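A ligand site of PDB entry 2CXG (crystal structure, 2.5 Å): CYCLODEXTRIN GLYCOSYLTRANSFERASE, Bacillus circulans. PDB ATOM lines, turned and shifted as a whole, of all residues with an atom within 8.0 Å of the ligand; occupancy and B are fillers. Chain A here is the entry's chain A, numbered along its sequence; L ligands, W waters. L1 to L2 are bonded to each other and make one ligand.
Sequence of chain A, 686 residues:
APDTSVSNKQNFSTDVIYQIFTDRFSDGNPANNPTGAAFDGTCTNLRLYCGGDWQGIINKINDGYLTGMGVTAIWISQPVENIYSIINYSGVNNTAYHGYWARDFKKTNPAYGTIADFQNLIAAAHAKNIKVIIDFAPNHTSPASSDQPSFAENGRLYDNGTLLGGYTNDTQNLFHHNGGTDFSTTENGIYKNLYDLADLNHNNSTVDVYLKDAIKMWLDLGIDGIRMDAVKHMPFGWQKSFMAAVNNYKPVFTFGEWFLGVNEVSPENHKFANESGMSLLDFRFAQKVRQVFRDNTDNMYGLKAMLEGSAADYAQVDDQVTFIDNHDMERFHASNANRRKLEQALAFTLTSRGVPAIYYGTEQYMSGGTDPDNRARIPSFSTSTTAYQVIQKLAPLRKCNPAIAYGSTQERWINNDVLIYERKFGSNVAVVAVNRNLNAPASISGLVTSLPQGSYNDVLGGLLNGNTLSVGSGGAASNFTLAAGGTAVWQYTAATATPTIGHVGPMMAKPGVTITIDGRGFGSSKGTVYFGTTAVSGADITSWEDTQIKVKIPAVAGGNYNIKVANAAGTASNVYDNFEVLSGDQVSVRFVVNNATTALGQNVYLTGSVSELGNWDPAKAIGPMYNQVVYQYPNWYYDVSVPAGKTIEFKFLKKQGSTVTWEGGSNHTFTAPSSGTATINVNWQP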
ATOM      1  N   TYR A 301     -11.578   7.669  19.641  1.00  0.00           N
ATOM      2  CA  TYR A 301     -12.908   7.337  20.103  1.00  0.00           C
ATOM      3  C   TYR A 301     -13.843   7.079  18.930  1.00  0.00           C
ATOM      4  O   TYR A 301     -14.749   6.246  19.010  1.00  0.00           O
ATOM      5  CB  TYR A 301     -13.476   8.341  21.117  1.00  0.00           C
ATOM      6  CG  TYR A 301     -12.711   8.326  22.431  1.00  0.00           C
ATOM      7  CD1 TYR A 301     -12.928   7.329  23.390  1.00  0.00           C
ATOM      8  CD2 TYR A 301     -11.757   9.304  22.704  1.00  0.00           C
ATOM      9  CE1 TYR A 301     -12.219   7.309  24.588  1.00  0.00           C
ATOM     10  CE2 TYR A 301     -11.036   9.293  23.898  1.00  0.00           C
ATOM     11  CZ  TYR A 301     -11.270   8.309  24.836  1.00  0.00           C
ATOM     12  OH  TYR A 301     -10.520   8.367  25.967  1.00  0.00           O
ATOM     13  N   LYS A 304     -13.073   3.616  17.483  1.00  0.00           N
ATOM     14  CA  LYS A 304     -13.649   2.588  18.318  1.00  0.00           C
ATOM     15  C   LYS A 304     -15.134   2.441  18.067  1.00  0.00           C
ATOM     16  O   LYS A 304     -15.672   1.336  18.014  1.00  0.00           O
ATOM     17  CB  LYS A 304     -13.352   2.804  19.787  1.00  0.00           C
ATOM     18  CG  LYS A 304     -14.293   2.070  20.724  1.00  0.00           C
ATOM     19  CD  LYS A 304     -13.940   2.270  22.183  1.00  0.00           C
ATOM     20  CE  LYS A 304     -15.138   2.122  23.114  1.00  0.00           C
ATOM     21  NZ  LYS A 304     -14.918   1.160  24.198  1.00  0.00           N
ATOM     22  N   GLN A 410     -11.718  -6.031  20.317  1.00  0.00           N
ATOM     23  CA  GLN A 410     -11.979  -5.494  21.631  1.00  0.00           C
ATOM     24  C   GLN A 410     -10.997  -4.403  22.026  1.00  0.00           C
ATOM     25  O   GLN A 410      -9.787  -4.591  21.990  1.00  0.00           O
ATOM     26  CB  GLN A 410     -12.004  -6.613  22.676  1.00  0.00           C
ATOM     27  CG  GLN A 410     -12.564  -6.180  24.040  1.00  0.00           C
ATOM     28  CD  GLN A 410     -12.417  -7.261  25.090  1.00  0.00           C
ATOM     29  OE1 GLN A 410     -12.272  -6.991  26.286  1.00  0.00           O
ATOM     30  NE2 GLN A 410     -12.482  -8.517  24.630  1.00  0.00           N
ATOM     31  N   GLU A 411     -11.542  -3.256  22.391  1.00  0.00           N
ATOM     32  CA  GLU A 411     -10.734  -2.158  22.841  1.00  0.00           C
ATOM     33  C   GLU A 411     -10.189  -2.508  24.208  1.00  0.00           C
ATOM     34  O   GLU A 411     -10.938  -2.920  25.091  1.00  0.00           O
ATOM     35  CB  GLU A 411     -11.542  -0.851  22.902  1.00  0.00           C
ATOM     36  CG  GLU A 411     -10.773   0.315  23.539  1.00  0.00           C
ATOM     37  CD  GLU A 411     -11.054   0.458  24.997  1.00  0.00           C
ATOM     38  OE1 GLU A 411     -12.173   0.450  25.476  1.00  0.00           O
ATOM     39  OE2 GLU A 411      -9.963   0.616  25.716  1.00  0.00           O
ATOM     40  N   ARG A 412      -8.889  -2.377  24.406  1.00  0.00           N
ATOM     41  CA  ARG A 412      -8.308  -2.708  25.688  1.00  0.00           C
ATOM     42  C   ARG A 412      -7.711  -1.507  26.395  1.00  0.00           C
ATOM     43  O   ARG A 412      -7.491  -1.518  27.608  1.00  0.00           O
ATOM     44  CB  ARG A 412      -7.330  -3.869  25.589  1.00  0.00           C
ATOM     45  CG  ARG A 412      -7.978  -5.111  24.979  1.00  0.00           C
ATOM     46  CD  ARG A 412      -7.638  -6.389  25.739  1.00  0.00           C
ATOM     47  NE  ARG A 412      -8.542  -6.610  26.864  1.00  0.00           N
ATOM     48  CZ  ARG A 412      -8.963  -7.808  27.313  1.00  0.00           C
ATOM     49  NH1 ARG A 412      -8.581  -8.957  26.747  1.00  0.00           N
ATOM     50  NH2 ARG A 412      -9.759  -7.834  28.353  1.00  0.00           N
ATOM     51  N   TRP A 413      -7.491  -0.452  25.612  1.00  0.00           N
ATOM     52  CA  TRP A 413      -6.920   0.803  26.077  1.00  0.00           C
ATOM     53  C   TRP A 413      -7.197   1.862  25.028  1.00  0.00           C
ATOM     54  O   TRP A 413      -7.014   1.620  23.837  1.00  0.00           O
ATOM     55  CB  TRP A 413      -5.406   0.635  26.273  1.00  0.00           C
ATOM     56  CG  TRP A 413      -4.827   1.429  27.399  1.00  0.00           C
ATOM     57  CD1 TRP A 413      -4.613   0.986  28.665  1.00  0.00           C
ATOM     58  CD2 TRP A 413      -4.318   2.766  27.368  1.00  0.00           C
ATOM     59  NE1 TRP A 413      -4.036   1.960  29.426  1.00  0.00           N
ATOM     60  CE2 TRP A 413      -3.842   3.066  28.654  1.00  0.00           C
ATOM     61  CE3 TRP A 413      -4.224   3.732  26.370  1.00  0.00           C
ATOM     62  CZ2 TRP A 413      -3.289   4.309  28.954  1.00  0.00           C
ATOM     63  CZ3 TRP A 413      -3.682   4.967  26.674  1.00  0.00           C
ATOM     64  CH2 TRP A 413      -3.220   5.249  27.959  1.00  0.00           C
ATOM     65  N   ILE A 414      -7.658   3.037  25.446  1.00  0.00           N
ATOM     66  CA  ILE A 414      -7.958   4.044  24.468  1.00  0.00           C
ATOM     67  C   ILE A 414      -7.845   5.461  24.993  1.00  0.00           C
ATOM     68  O   ILE A 414      -7.979   5.714  26.196  1.00  0.00           O
ATOM     69  CB  ILE A 414      -9.344   3.841  23.849  1.00  0.00           C
ATOM     70  CG1 ILE A 414      -9.539   4.795  22.670  1.00  0.00           C
ATOM     71  CG2 ILE A 414     -10.413   4.098  24.899  1.00  0.00           C
ATOM     72  CD1 ILE A 414     -10.922   4.676  22.033  1.00  0.00           C
ATOM     73  N   ASN A 415      -7.655   6.370  24.055  1.00  0.00           N
ATOM     74  CA  ASN A 415      -7.575   7.779  24.331  1.00  0.00           C
ATOM     75  C   ASN A 415      -7.568   8.503  23.004  1.00  0.00           C
ATOM     76  O   ASN A 415      -7.320   7.856  21.999  1.00  0.00           O
ATOM     77  CB  ASN A 415      -6.382   8.103  25.261  1.00  0.00           C
ATOM     78  CG  ASN A 415      -5.086   8.620  24.634  1.00  0.00           C
ATOM     79  OD1 ASN A 415      -4.819   8.542  23.440  1.00  0.00           O
ATOM     80  ND2 ASN A 415      -4.229   9.103  25.487  1.00  0.00           N
ATOM     81  N   ASN A 416      -7.645   9.836  23.027  1.00  0.00           N
ATOM     82  CA  ASN A 416      -7.607  10.706  21.855  1.00  0.00           C
ATOM     83  C   ASN A 416      -6.689  10.238  20.729  1.00  0.00           C
ATOM     84  O   ASN A 416      -7.131  10.115  19.601  1.00  0.00           O
ATOM     85  CB  ASN A 416      -7.186  12.118  22.252  1.00  0.00           C
ATOM     86  CG  ASN A 416      -8.357  13.030  22.511  1.00  0.00           C
ATOM     87  OD1 ASN A 416      -9.517  12.635  22.375  1.00  0.00           O
ATOM     88  ND2 ASN A 416      -8.043  14.240  22.947  1.00  0.00           N
ATOM     89  N   VAL A 418      -4.373   7.310  21.096  1.00  0.00           N
ATOM     90  CA  VAL A 418      -3.935   5.931  21.218  1.00  0.00           C
ATOM     91  C   VAL A 418      -5.060   4.927  21.118  1.00  0.00           C
ATOM     92  O   VAL A 418      -6.166   5.138  21.599  1.00  0.00           O
ATOM     93  CB  VAL A 418      -3.148   5.686  22.495  1.00  0.00           C
ATOM     94  CG1 VAL A 418      -2.742   4.218  22.584  1.00  0.00           C
ATOM     95  CG2 VAL A 418      -1.906   6.568  22.541  1.00  0.00           C
ATOM     96  N   ILE A 420      -5.489   0.571  21.429  1.00  0.00           N
ATOM     97  CA  ILE A 420      -5.010  -0.785  21.633  1.00  0.00           C
ATOM     98  C   ILE A 420      -6.171  -1.760  21.550  1.00  0.00           C
ATOM     99  O   ILE A 420      -7.147  -1.647  22.294  1.00  0.00           O
ATOM    100  CB  ILE A 420      -4.253  -0.943  22.947  1.00  0.00           C
ATOM    101  CG1 ILE A 420      -3.203   0.150  23.092  1.00  0.00           C
ATOM    102  CG2 ILE A 420      -3.580  -2.309  22.994  1.00  0.00           C
ATOM    103  CD1 ILE A 420      -1.994  -0.289  23.916  1.00  0.00           C
ATOM    104  N   SER A 443       2.087   7.013  27.851  1.00  0.00           N
ATOM    105  CA  SER A 443       2.365   6.103  28.923  1.00  0.00           C
ATOM    106  C   SER A 443       1.198   5.150  29.086  1.00  0.00           C
ATOM    107  O   SER A 443       0.073   5.560  29.355  1.00  0.00           O
ATOM    108  CB  SER A 443       2.739   6.818  30.214  1.00  0.00           C
ATOM    109  OG  SER A 443       1.726   6.646  31.186  1.00  0.00           O
ATOM    110  N   ILE A 444       1.463   3.878  28.843  1.00  0.00           N
ATOM    111  CA  ILE A 444       0.410   2.898  28.943  1.00  0.00           C
ATOM    112  C   ILE A 444       0.475   2.053  30.193  1.00  0.00           C
ATOM    113  O   ILE A 444       1.354   1.213  30.349  1.00  0.00           O
ATOM    114  CB  ILE A 444       0.242   2.051  27.691  1.00  0.00           C
ATOM    115  CG1 ILE A 444      -0.471   2.870  26.613  1.00  0.00           C
ATOM    116  CG2 ILE A 444      -0.590   0.808  28.018  1.00  0.00           C
ATOM    117  CD1 ILE A 444       0.483   3.463  25.589  1.00  0.00           C
ATOM    118  N   SER A 445      -0.488   2.303  31.071  1.00  0.00           N
ATOM    119  CA  SER A 445      -0.625   1.581  32.302  1.00  0.00           C
ATOM    120  C   SER A 445      -2.050   1.084  32.419  1.00  0.00           C
ATOM    121  O   SER A 445      -2.970   1.744  31.938  1.00  0.00           O
ATOM    122  CB  SER A 445      -0.244   2.424  33.514  1.00  0.00           C
ATOM    123  OG  SER A 445      -0.763   3.724  33.376  1.00  0.00           O
ATOM    124  N   GLY A 446      -2.225  -0.079  33.027  1.00  0.00           N
ATOM    125  CA  GLY A 446      -3.540  -0.658  33.204  1.00  0.00           C
ATOM    126  C   GLY A 446      -3.975  -1.574  32.058  1.00  0.00           C
ATOM    127  O   GLY A 446      -5.109  -2.043  32.038  1.00  0.00           O
ATOM    128  N   LEU A 447      -3.054  -1.823  31.128  1.00  0.00           N
ATOM    129  CA  LEU A 447      -3.342  -2.691  29.984  1.00  0.00           C
ATOM    130  C   LEU A 447      -3.552  -4.139  30.393  1.00  0.00           C
ATOM    131  O   LEU A 447      -2.706  -4.747  31.049  1.00  0.00           O
ATOM    132  CB  LEU A 447      -2.281  -2.573  28.869  1.00  0.00           C
ATOM    133  CG  LEU A 447      -2.504  -3.568  27.735  1.00  0.00           C
ATOM    134  CD1 LEU A 447      -3.781  -3.219  26.976  1.00  0.00           C
ATOM    135  CD2 LEU A 447      -1.301  -3.551  26.787  1.00  0.00           C
ATOM    136  N   VAL A 448      -4.688  -4.674  29.978  1.00  0.00           N
ATOM    137  CA  VAL A 448      -5.054  -6.051  30.283  1.00  0.00           C
ATOM    138  C   VAL A 448      -5.346  -6.809  29.000  1.00  0.00           C
ATOM    139  O   VAL A 448      -6.116  -6.350  28.161  1.00  0.00           O
ATOM    140  CB  VAL A 448      -6.229  -6.114  31.238  1.00  0.00           C
ATOM    141  CG1 VAL A 448      -6.582  -7.559  31.533  1.00  0.00           C
ATOM    142  CG2 VAL A 448      -5.863  -5.398  32.536  1.00  0.00           C
HETATM  143  C1  LIG L   1      -6.468   5.195  30.950  1.00  0.00           C
HETATM  144  C2  LIG L   1      -6.833   4.733  29.573  1.00  0.00           C
HETATM  145  C3  LIG L   1      -7.926   3.705  29.658  1.00  0.00           C
HETATM  146  C4  LIG L   1      -7.405   2.534  30.474  1.00  0.00           C
HETATM  147  C5  LIG L   1      -6.948   3.020  31.852  1.00  0.00           C
HETATM  148  C6  LIG L   1      -6.234   1.935  32.616  1.00  0.00           C
HETATM  149  O1  LIG L   1      -7.564   5.811  31.512  1.00  0.00           O
HETATM  150  O2  LIG L   1      -7.295   5.845  28.801  1.00  0.00           O
HETATM  151  O3  LIG L   1      -8.287   3.343  28.343  1.00  0.00           O
HETATM  152  O4  LIG L   1      -8.511   1.625  30.646  1.00  0.00           O
HETATM  153  O5  LIG L   1      -5.994   4.074  31.706  1.00  0.00           O
HETATM  154  O6  LIG L   1      -7.065   1.540  33.715  1.00  0.00           O
HETATM  155  C1  LG2 L   2      -8.441   0.361  30.020  1.00  0.00           C
HETATM  156  C2  LG2 L   2      -9.742   0.085  29.304  1.00  0.00           C
HETATM  157  C3  LG2 L   2     -10.873  -0.226  30.249  1.00  0.00           C
HETATM  158  C4  LG2 L   2     -10.487  -1.230  31.319  1.00  0.00           C
HETATM  159  C5  LG2 L   2      -9.152  -0.899  31.945  1.00  0.00           C
HETATM  160  C6  LG2 L   2      -8.652  -2.019  32.796  1.00  0.00           C
HETATM  161  O1  LG2 L   2     -10.072   1.200  28.488  1.00  0.00           O
HETATM  162  O2  LG2 L   2     -11.999  -0.758  29.544  1.00  0.00           O
HETATM  163  O3  LG2 L   2     -11.429  -1.201  32.379  1.00  0.00           O
HETATM  164  O4  LG2 L   2      -8.141  -0.674  30.952  1.00  0.00           O
HETATM  165  O5  LG2 L   2      -7.470  -1.653  33.535  1.00  0.00           O
HETATM  166  O   HOH W   1      -2.966   5.104  31.897  1.00  0.00           O
HETATM  167  O   HOH W   2     -10.483   6.543  27.916  1.00  0.00           O
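The backbone NH of Ile 414 is in hydrogen-bond range of an oxygen (O3) of LIG L1 (3.0 Å). The backbone carbonyl oxygen (O) of Ile 414 lies within hydrogen-bond range of an oxygen (O2) of LIG L1. An oxygen (O5) of LG2 L2 sits at hydrogen-bond distance from the backbone carbonyl oxygen (O) of Gly 446. The side-chain carboxylate of Glu 411 sits at hydrogen-bond distance from an oxygen (O1) of LG2 L2 (2.8 Å).
N of Ile 414 is in hydrogen-bond range of OE2 of Glu 411, at 3.4 Å. The backbone NH (N) of Trp 413 lies within hydrogen-bond range of the side-chain carboxylate (OE2) of Glu 411 (2.7 Å). The side-chain carboxylate of Glu 411 lies within salt-bridge range of the side-chain amino group of Lys 304, at 3.1 Å. The guanidinium group (NE) of Arg 412 sits at hydrogen-bond distance from the backbone carbonyl oxygen (O) of Val 448 (2.8 Å). The guanidinium group (NH2) of Arg 412 sits at hydrogen-bond distance from the side-chain amide oxygen (OE1) of Gln 410, 3.4 Å away. The backbone carbonyl oxygen (O) of Ile 420 sits at hydrogen-bond distance from the backbone NH (N) of Arg 412, at 2.8 Å. The indole nitrogen (NE1) of Trp 413 sits at hydrogen-bond distance from the backbone carbonyl oxygen (O) of Ser 445. O of Trp 413 lies within hydrogen-bond range of N of Ile 420 (3.0 Å).
O of Arg 412 touches C1 of LG2 L2, at 3.2 Å. Trp 413 touches the ligand. O of Ser 445 touches C6 of LIG L1 (3.3 Å). Within 4 Å of the ligand: Glu 411, Arg 412, Trp 413, Ile 414, Ser 445 and Gly 446.
Water W1 bridges OG of Ser 445 (3.0 Å) and O5 of LIG L1 (3.2 Å). Water W2 lies within hydrogen-bond range of OH of Tyr 301, O of Ile 414 and O2 of LIG L1.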
